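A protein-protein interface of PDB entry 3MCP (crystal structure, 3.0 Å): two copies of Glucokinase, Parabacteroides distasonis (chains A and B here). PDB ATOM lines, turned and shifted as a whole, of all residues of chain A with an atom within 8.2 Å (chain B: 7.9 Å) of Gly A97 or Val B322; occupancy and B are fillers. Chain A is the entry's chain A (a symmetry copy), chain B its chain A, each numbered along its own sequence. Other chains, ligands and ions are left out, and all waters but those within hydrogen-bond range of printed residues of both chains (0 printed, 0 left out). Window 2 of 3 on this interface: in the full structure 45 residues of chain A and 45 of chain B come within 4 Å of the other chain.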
ATOM      1  N   PRO A  77      19.083 -13.368  24.340  1.00  0.00           N
ATOM      2  CA  PRO A  77      19.176 -13.095  22.904  1.00  0.00           C
ATOM      3  C   PRO A  77      17.842 -13.010  22.224  1.00  0.00           C
ATOM      4  O   PRO A  77      16.896 -13.678  22.632  1.00  0.00           O
ATOM      5  CB  PRO A  77      19.928 -14.314  22.373  1.00  0.00           C
ATOM      6  CG  PRO A  77      19.502 -15.403  23.257  1.00  0.00           C
ATOM      7  CD  PRO A  77      19.424 -14.771  24.634  1.00  0.00           C
ATOM      8  N   ALA A  82      13.185  -7.629  14.466  1.00  0.00           N
ATOM      9  CA  ALA A  82      11.933  -8.331  14.174  1.00  0.00           C
ATOM     10  C   ALA A  82      11.020  -8.359  15.410  1.00  0.00           C
ATOM     11  O   ALA A  82       9.836  -8.670  15.311  1.00  0.00           O
ATOM     12  CB  ALA A  82      12.224  -9.750  13.697  1.00  0.00           C
ATOM     13  N   GLY A  83      11.589  -8.063  16.574  1.00  0.00           N
ATOM     14  CA  GLY A  83      10.829  -8.020  17.809  1.00  0.00           C
ATOM     15  C   GLY A  83      10.406  -9.384  18.324  1.00  0.00           C
ATOM     16  O   GLY A  83       9.409  -9.501  19.023  1.00  0.00           O
ATOM     17  N   ILE A  84      11.158 -10.420  17.986  1.00  0.00           N
ATOM     18  CA  ILE A  84      10.844 -11.758  18.483  1.00  0.00           C
ATOM     19  C   ILE A  84      12.006 -12.261  19.344  1.00  0.00           C
ATOM     20  O   ILE A  84      13.159 -12.233  18.931  1.00  0.00           O
ATOM     21  CB  ILE A  84      10.467 -12.730  17.329  1.00  0.00           C
ATOM     22  CG1 ILE A  84      11.657 -13.115  16.505  1.00  0.00           C
ATOM     23  CG2 ILE A  84       9.454 -12.071  16.389  1.00  0.00           C
ATOM     24  CD1 ILE A  84      11.254 -13.567  15.109  1.00  0.00           C
ATOM     25  N   ILE A  85      11.677 -12.681  20.563  1.00  0.00           N
ATOM     26  CA  ILE A  85      12.671 -12.994  21.588  1.00  0.00           C
ATOM     27  C   ILE A  85      13.028 -14.464  21.644  1.00  0.00           C
ATOM     28  O   ILE A  85      12.174 -15.318  21.490  1.00  0.00           O
ATOM     29  CB  ILE A  85      12.153 -12.576  22.949  1.00  0.00           C
ATOM     30  CG1 ILE A  85      11.805 -11.084  22.928  1.00  0.00           C
ATOM     31  CG2 ILE A  85      13.183 -12.873  24.032  1.00  0.00           C
ATOM     32  CD1 ILE A  85      10.960 -10.651  24.085  1.00  0.00           C
ATOM     33  N   GLY A  86      14.296 -14.746  21.930  1.00  0.00           N
ATOM     34  CA  GLY A  86      14.807 -16.115  21.948  1.00  0.00           C
ATOM     35  C   GLY A  86      14.656 -16.842  23.276  1.00  0.00           C
ATOM     36  O   GLY A  86      13.909 -16.418  24.157  1.00  0.00           O
ATOM     37  N   ASP A  87      15.387 -17.946  23.410  1.00  0.00           N
ATOM     38  CA  ASP A  87      15.309 -18.791  24.593  1.00  0.00           C
ATOM     39  C   ASP A  87      16.042 -18.157  25.772  1.00  0.00           C
ATOM     40  O   ASP A  87      17.242 -18.346  25.942  1.00  0.00           O
ATOM     41  CB  ASP A  87      15.901 -20.183  24.290  1.00  0.00           C
ATOM     42  CG  ASP A  87      15.153 -20.919  23.159  1.00  0.00           C
ATOM     43  OD1 ASP A  87      14.332 -20.278  22.454  1.00  0.00           O
ATOM     44  OD2 ASP A  87      15.397 -22.138  22.977  1.00  0.00           O
ATOM     45  N   LEU A  88      15.313 -17.403  26.585  1.00  0.00           N
ATOM     46  CA  LEU A  88      15.902 -16.772  27.759  1.00  0.00           C
ATOM     47  C   LEU A  88      16.039 -17.789  28.875  1.00  0.00           C
ATOM     48  O   LEU A  88      15.151 -18.622  29.070  1.00  0.00           O
ATOM     49  CB  LEU A  88      15.039 -15.613  28.244  1.00  0.00           C
ATOM     50  CG  LEU A  88      14.739 -14.519  27.225  1.00  0.00           C
ATOM     51  CD1 LEU A  88      13.871 -13.446  27.841  1.00  0.00           C
ATOM     52  CD2 LEU A  88      16.011 -13.930  26.711  1.00  0.00           C
ATOM     53  N   SER A  93       8.997 -20.187  29.856  1.00  0.00           N
ATOM     54  CA  SER A  93       7.887 -20.244  28.886  1.00  0.00           C
ATOM     55  C   SER A  93       8.234 -19.541  27.575  1.00  0.00           C
ATOM     56  O   SER A  93       7.342 -19.250  26.778  1.00  0.00           O
ATOM     57  CB  SER A  93       6.619 -19.624  29.477  1.00  0.00           C
ATOM     58  N   PHE A  94       9.533 -19.298  27.350  1.00  0.00           N
ATOM     59  CA  PHE A  94      10.017 -18.570  26.161  1.00  0.00           C
ATOM     60  C   PHE A  94      10.814 -19.410  25.168  1.00  0.00           C
ATOM     61  O   PHE A  94      11.203 -18.913  24.108  1.00  0.00           O
ATOM     62  CB  PHE A  94      10.859 -17.366  26.589  1.00  0.00           C
ATOM     63  CG  PHE A  94      10.094 -16.068  26.614  1.00  0.00           C
ATOM     64  CD1 PHE A  94       9.022 -15.892  27.479  1.00  0.00           C
ATOM     65  CD2 PHE A  94      10.460 -15.014  25.785  1.00  0.00           C
ATOM     66  CE1 PHE A  94       8.322 -14.695  27.504  1.00  0.00           C
ATOM     67  CE2 PHE A  94       9.768 -13.818  25.813  1.00  0.00           C
ATOM     68  CZ  PHE A  94       8.698 -13.659  26.671  1.00  0.00           C
ATOM     69  N   ARG A  95      11.064 -20.670  25.498  1.00  0.00           N
ATOM     70  CA  ARG A  95      11.782 -21.555  24.578  1.00  0.00           C
ATOM     71  C   ARG A  95      10.967 -21.707  23.274  1.00  0.00           C
ATOM     72  O   ARG A  95       9.754 -21.930  23.316  1.00  0.00           O
ATOM     73  CB  ARG A  95      12.059 -22.930  25.231  1.00  0.00           C
ATOM     74  CG  ARG A  95      13.277 -22.960  26.218  1.00  0.00           C
ATOM     75  CD  ARG A  95      13.231 -21.831  27.270  1.00  0.00           C
ATOM     76  NE  ARG A  95      14.215 -22.022  28.339  1.00  0.00           N
ATOM     77  CZ  ARG A  95      15.475 -21.594  28.284  1.00  0.00           C
ATOM     78  N   GLY A  96      11.627 -21.511  22.128  1.00  0.00           N
ATOM     79  CA  GLY A  96      10.970 -21.657  20.814  1.00  0.00           C
ATOM     80  C   GLY A  96      11.056 -20.420  19.928  1.00  0.00           C
ATOM     81  O   GLY A  96      11.322 -20.526  18.721  1.00  0.00           O
ATOM     82  N   GLY A  97      10.829 -19.249  20.526  1.00  0.00           N
ATOM     83  CA  GLY A  97      10.815 -17.978  19.791  1.00  0.00           C
ATOM     84  C   GLY A  97       9.471 -17.300  19.952  1.00  0.00           C
ATOM     85  O   GLY A  97       8.486 -17.721  19.359  1.00  0.00           O
ATOM     86  N   VAL A  98       9.427 -16.256  20.771  1.00  0.00           N
ATOM     87  CA  VAL A  98       8.182 -15.541  21.048  1.00  0.00           C
ATOM     88  C   VAL A  98       8.139 -14.233  20.296  1.00  0.00           C
ATOM     89  O   VAL A  98       8.956 -13.357  20.539  1.00  0.00           O
ATOM     90  CB  VAL A  98       8.036 -15.233  22.554  1.00  0.00           C
ATOM     91  CG1 VAL A  98       6.771 -14.424  22.818  1.00  0.00           C
ATOM     92  CG2 VAL A  98       8.033 -16.517  23.366  1.00  0.00           C
ATOM     93  N   ALA A  99       7.167 -14.092  19.394  1.00  0.00           N
ATOM     94  CA  ALA A  99       7.003 -12.857  18.621  1.00  0.00           C
ATOM     95  C   ALA A  99       6.349 -11.787  19.482  1.00  0.00           C
ATOM     96  O   ALA A  99       5.212 -11.382  19.246  1.00  0.00           O
ATOM     97  CB  ALA A  99       6.188 -13.114  17.373  1.00  0.00           C
ATOM     98  N   LEU A 100       7.100 -11.310  20.465  1.00  0.00           N
ATOM     99  CA  LEU A 100       6.593 -10.351  21.428  1.00  0.00           C
ATOM    100  C   LEU A 100       6.292  -9.002  20.789  1.00  0.00           C
ATOM    101  O   LEU A 100       5.264  -8.394  21.068  1.00  0.00           O
ATOM    102  CB  LEU A 100       7.595 -10.193  22.575  1.00  0.00           C
ATOM    103  CG  LEU A 100       7.274  -9.168  23.657  1.00  0.00           C
ATOM    104  CD1 LEU A 100       5.840  -9.290  24.111  1.00  0.00           C
ATOM    105  CD2 LEU A 100       8.236  -9.325  24.836  1.00  0.00           C
ATOM    106  N   PRO A 102       5.526  -8.033  17.488  1.00  0.00           N
ATOM    107  CA  PRO A 102       4.290  -8.093  16.701  1.00  0.00           C
ATOM    108  C   PRO A 102       3.029  -8.326  17.551  1.00  0.00           C
ATOM    109  O   PRO A 102       1.964  -7.788  17.242  1.00  0.00           O
ATOM    110  CB  PRO A 102       4.527  -9.285  15.779  1.00  0.00           C
ATOM    111  CG  PRO A 102       6.000  -9.338  15.608  1.00  0.00           C
ATOM    112  CD  PRO A 102       6.589  -8.873  16.903  1.00  0.00           C
ATOM    113  N   ALA B 319      16.338 -22.179  10.899  1.00  0.00           N
ATOM    114  CA  ALA B 319      15.198 -21.330  10.505  1.00  0.00           C
ATOM    115  C   ALA B 319      13.839 -21.984  10.751  1.00  0.00           C
ATOM    116  O   ALA B 319      13.650 -23.167  10.463  1.00  0.00           O
ATOM    117  CB  ALA B 319      15.326 -20.940   9.032  1.00  0.00           C
ATOM    118  N   VAL B 320      12.891 -21.192  11.257  1.00  0.00           N
ATOM    119  CA  VAL B 320      11.519 -21.661  11.504  1.00  0.00           C
ATOM    120  C   VAL B 320      10.509 -20.526  11.287  1.00  0.00           C
ATOM    121  O   VAL B 320      10.874 -19.428  10.877  1.00  0.00           O
ATOM    122  CB  VAL B 320      11.344 -22.196  12.965  1.00  0.00           C
ATOM    123  CG1 VAL B 320      12.275 -23.360  13.233  1.00  0.00           C
ATOM    124  CG2 VAL B 320      11.569 -21.088  13.971  1.00  0.00           C
ATOM    125  N   GLU B 321       9.234 -20.822  11.519  1.00  0.00           N
ATOM    126  CA  GLU B 321       8.187 -19.804  11.531  1.00  0.00           C
ATOM    127  C   GLU B 321       7.507 -19.861  12.887  1.00  0.00           C
ATOM    128  O   GLU B 321       7.250 -20.945  13.407  1.00  0.00           O
ATOM    129  CB  GLU B 321       7.147 -20.053  10.432  1.00  0.00           C
ATOM    130  CG  GLU B 321       7.612 -19.755   9.000  1.00  0.00           C
ATOM    131  CD  GLU B 321       6.462 -19.845   7.987  1.00  0.00           C
ATOM    132  OE1 GLU B 321       5.348 -19.363   8.295  1.00  0.00           O
ATOM    133  OE2 GLU B 321       6.674 -20.394   6.887  1.00  0.00           O
ATOM    134  N   VAL B 322       7.224 -18.700  13.466  1.00  0.00           N
ATOM    135  CA  VAL B 322       6.547 -18.645  14.762  1.00  0.00           C
ATOM    136  C   VAL B 322       5.231 -17.912  14.630  1.00  0.00           C
ATOM    137  O   VAL B 322       5.132 -16.910  13.935  1.00  0.00           O
ATOM    138  CB  VAL B 322       7.415 -17.968  15.855  1.00  0.00           C
ATOM    139  CG1 VAL B 322       8.650 -18.805  16.147  1.00  0.00           C
ATOM    140  CG2 VAL B 322       7.798 -16.561  15.443  1.00  0.00           C
ATOM    141  N   LEU B 323       4.218 -18.436  15.295  1.00  0.00           N
ATOM    142  CA  LEU B 323       2.893 -17.873  15.231  1.00  0.00           C
ATOM    143  C   LEU B 323       2.815 -16.668  16.156  1.00  0.00           C
ATOM    144  O   LEU B 323       3.296 -16.718  17.289  1.00  0.00           O
ATOM    145  CB  LEU B 323       1.855 -18.934  15.649  1.00  0.00           C
ATOM    146  CG  LEU B 323       0.388 -18.661  15.289  1.00  0.00           C
ATOM    147  CD1 LEU B 323       0.166 -18.792  13.779  1.00  0.00           C
ATOM    148  CD2 LEU B 323      -0.541 -19.610  16.053  1.00  0.00           C
ATOM    149  N   VAL B 324       2.246 -15.573  15.656  1.00  0.00           N
ATOM    150  CA  VAL B 324       2.024 -14.383  16.470  1.00  0.00           C
ATOM    151  C   VAL B 324       0.876 -14.682  17.436  1.00  0.00           C
ATOM    152  O   VAL B 324      -0.278 -14.790  17.014  1.00  0.00           O
ATOM    153  CB  VAL B 324       1.655 -13.163  15.606  1.00  0.00           C
ATOM    154  CG1 VAL B 324       1.385 -11.957  16.482  1.00  0.00           C
ATOM    155  CG2 VAL B 324       2.758 -12.864  14.615  1.00  0.00           C
ATOM    156  N   PRO B 325       1.194 -14.834  18.740  1.00  0.00           N
ATOM    157  CA  PRO B 325       0.204 -15.205  19.758  1.00  0.00           C
ATOM    158  C   PRO B 325      -1.164 -14.539  19.567  1.00  0.00           C
ATOM    159  O   PRO B 325      -1.250 -13.313  19.474  1.00  0.00           O
ATOM    160  CB  PRO B 325       0.854 -14.730  21.056  1.00  0.00           C
ATOM    161  CG  PRO B 325       2.306 -14.841  20.799  1.00  0.00           C
ATOM    162  CD  PRO B 325       2.505 -14.527  19.345  1.00  0.00           C
ATOM    163  N   ASN B 328      -3.571 -15.478  13.579  1.00  0.00           N
ATOM    164  CA  ASN B 328      -3.408 -16.627  12.686  1.00  0.00           C
ATOM    165  C   ASN B 328      -2.199 -16.418  11.768  1.00  0.00           C
ATOM    166  O   ASN B 328      -1.981 -17.198  10.830  1.00  0.00           O
ATOM    167  CB  ASN B 328      -4.674 -16.835  11.825  1.00  0.00           C
ATOM    168  CG  ASN B 328      -5.869 -17.368  12.634  1.00  0.00           C
ATOM    169  OD1 ASN B 328      -5.727 -17.789  13.788  1.00  0.00           O
ATOM    170  ND2 ASN B 328      -7.047 -17.366  12.014  1.00  0.00           N
ATOM    171  N   ARG B 329      -1.401 -15.380  12.064  1.00  0.00           N
ATOM    172  CA  ARG B 329      -0.245 -14.996  11.233  1.00  0.00           C
ATOM    173  C   ARG B 329       1.032 -15.690  11.718  1.00  0.00           C
ATOM    174  O   ARG B 329       1.165 -15.988  12.902  1.00  0.00           O
ATOM    175  CB  ARG B 329      -0.018 -13.471  11.288  1.00  0.00           C
ATOM    176  CG  ARG B 329      -1.294 -12.595  11.345  1.00  0.00           C
ATOM    177  CD  ARG B 329      -0.938 -11.135  11.707  1.00  0.00           C
ATOM    178  NE  ARG B 329      -2.044 -10.440  12.360  1.00  0.00           N
ATOM    179  N   LYS B 330       1.971 -15.923  10.799  1.00  0.00           N
ATOM    180  CA  LYS B 330       3.275 -16.518  11.139  1.00  0.00           C
ATOM    181  C   LYS B 330       4.410 -15.546  10.779  1.00  0.00           C
ATOM    182  O   LYS B 330       4.327 -14.829   9.787  1.00  0.00           O
ATOM    183  CB  LYS B 330       3.471 -17.860  10.414  1.00  0.00           C
ATOM    184  CG  LYS B 330       2.565 -18.994  10.911  1.00  0.00           C
ATOM    185  N   VAL B 331       5.458 -15.520  11.605  1.00  0.00           N
ATOM    186  CA  VAL B 331       6.599 -14.618  11.396  1.00  0.00           C
ATOM    187  C   VAL B 331       7.896 -15.419  11.391  1.00  0.00           C
ATOM    188  O   VAL B 331       8.040 -16.372  12.152  1.00  0.00           O
ATOM    189  CB  VAL B 331       6.670 -13.540  12.497  1.00  0.00           C
ATOM    190  N   GLY B 332       8.836 -15.029  10.525  1.00  0.00           N
ATOM    191  CA  GLY B 332      10.114 -15.752  10.376  1.00  0.00           C
ATOM    192  C   GLY B 332      11.095 -15.505  11.518  1.00  0.00           C
ATOM    193  O   GLY B 332      11.203 -14.393  12.018  1.00  0.00           O
ATOM    194  N   TYR B 333      11.823 -16.547  11.910  1.00  0.00           N
ATOM    195  CA  TYR B 333      12.760 -16.458  13.026  1.00  0.00           C
ATOM    196  C   TYR B 333      13.829 -17.516  12.933  1.00  0.00           C
ATOM    197  O   TYR B 333      13.541 -18.683  12.662  1.00  0.00           O
ATOM    198  CB  TYR B 333      12.022 -16.622  14.357  1.00  0.00           C
ATOM    199  CG  TYR B 333      12.939 -16.703  15.586  1.00  0.00           C
ATOM    200  CD1 TYR B 333      13.782 -15.644  15.926  1.00  0.00           C
ATOM    201  CD2 TYR B 333      12.925 -17.825  16.422  1.00  0.00           C
ATOM    202  CE1 TYR B 333      14.607 -15.707  17.054  1.00  0.00           C
ATOM    203  CE2 TYR B 333      13.745 -17.897  17.551  1.00  0.00           C
ATOM    204  CZ  TYR B 333      14.582 -16.836  17.859  1.00  0.00           C
ATOM    205  OH  TYR B 333      15.395 -16.904  18.973  1.00  0.00           O
ATOM    206  N   ASP B 334      15.067 -17.112  13.197  1.00  0.00           N
ATOM    207  CA  ASP B 334      16.186 -18.022  13.197  1.00  0.00           C
ATOM    208  C   ASP B 334      17.090 -17.666  14.371  1.00  0.00           C
ATOM    209  O   ASP B 334      17.796 -16.668  14.324  1.00  0.00           O
ATOM    210  CB  ASP B 334      16.945 -17.915  11.875  1.00  0.00           C
ATOM    211  CG  ASP B 334      18.053 -18.949  11.743  1.00  0.00           C
ATOM    212  OD1 ASP B 334      18.273 -19.723  12.699  1.00  0.00           O
ATOM    213  OD2 ASP B 334      18.708 -18.979  10.678  1.00  0.00           O
ATOM    214  N   PRO B 335      17.055 -18.476  15.441  1.00  0.00           N
ATOM    215  CA  PRO B 335      17.868 -18.195  16.622  1.00  0.00           C
ATOM    216  C   PRO B 335      19.348 -18.455  16.392  1.00  0.00           C
ATOM    217  O   PRO B 335      20.174 -18.099  17.237  1.00  0.00           O
ATOM    218  CB  PRO B 335      17.332 -19.189  17.653  1.00  0.00           C
ATOM    219  CG  PRO B 335      16.918 -20.356  16.853  1.00  0.00           C
ATOM    220  CD  PRO B 335      16.419 -19.802  15.523  1.00  0.00           C
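N of Val B320 is in hydrogen-bond range of O of Tyr B333, 2.9 Å away. The side-chain carboxylate (OD1) of Asp A87 sits at hydrogen-bond distance from the backbone NH (N) of Gly A96, 3.0 Å away. The backbone carbonyl oxygen of Pro A77 lies within hydrogen-bond range of the backbone NH of Gly A86, at 2.9 Å. O of Val B322 sits at hydrogen-bond distance from N of Val B331 (2.7 Å).
Among the printed residues, pairs that only touch across the chains: Gly A86 with Tyr B333 (3.1 Å), Ile A84 with Gly B332 (3.2 Å), Ile A84 with Tyr B333 (3.2 Å), Gly A97 with Val B322 (3.4 Å), Gly A97 with Tyr B333 (3.7 Å) and Gly A96 with Tyr B333 (3.8 Å).
Printed residues of chain B within 4 Å of Gly A86: Tyr B333. Gly A96 touches one residue of chain B. Gly A97 touches two residues of chain B. Ala A99 touches none of the printed residues of chain B. Val B322 touches just one residue of chain A: Gly A97. No residue of chain A comes within 4 Å of Val B331. Printed residues of chain A within 4 Å of Gly B332: Ile A84 (3.2 Å). The nearest residue of chain B that does not touch Gly A97 is Leu B323 (5.7 Å). The nearest residue of chain A that does not touch Val B322 is Gly A96 (4.1 Å).
Of the 17 printed residues of chain A, 4 touch a printed residue of chain B. Hydrophobic or aromatic side chains of chain A that line the printed part of chain B: Ile A84. Hydrophobic or aromatic side chains of chain B that line the printed part of chain A: Val B322 and Tyr B333. Among the printed residues, 6 pairs touch across the chains. Among the printed residues, no Asp or Glu carboxylate lies within 4 Å of a Lys or Arg side-chain nitrogen of the other chain.
No position is printed for both chains.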
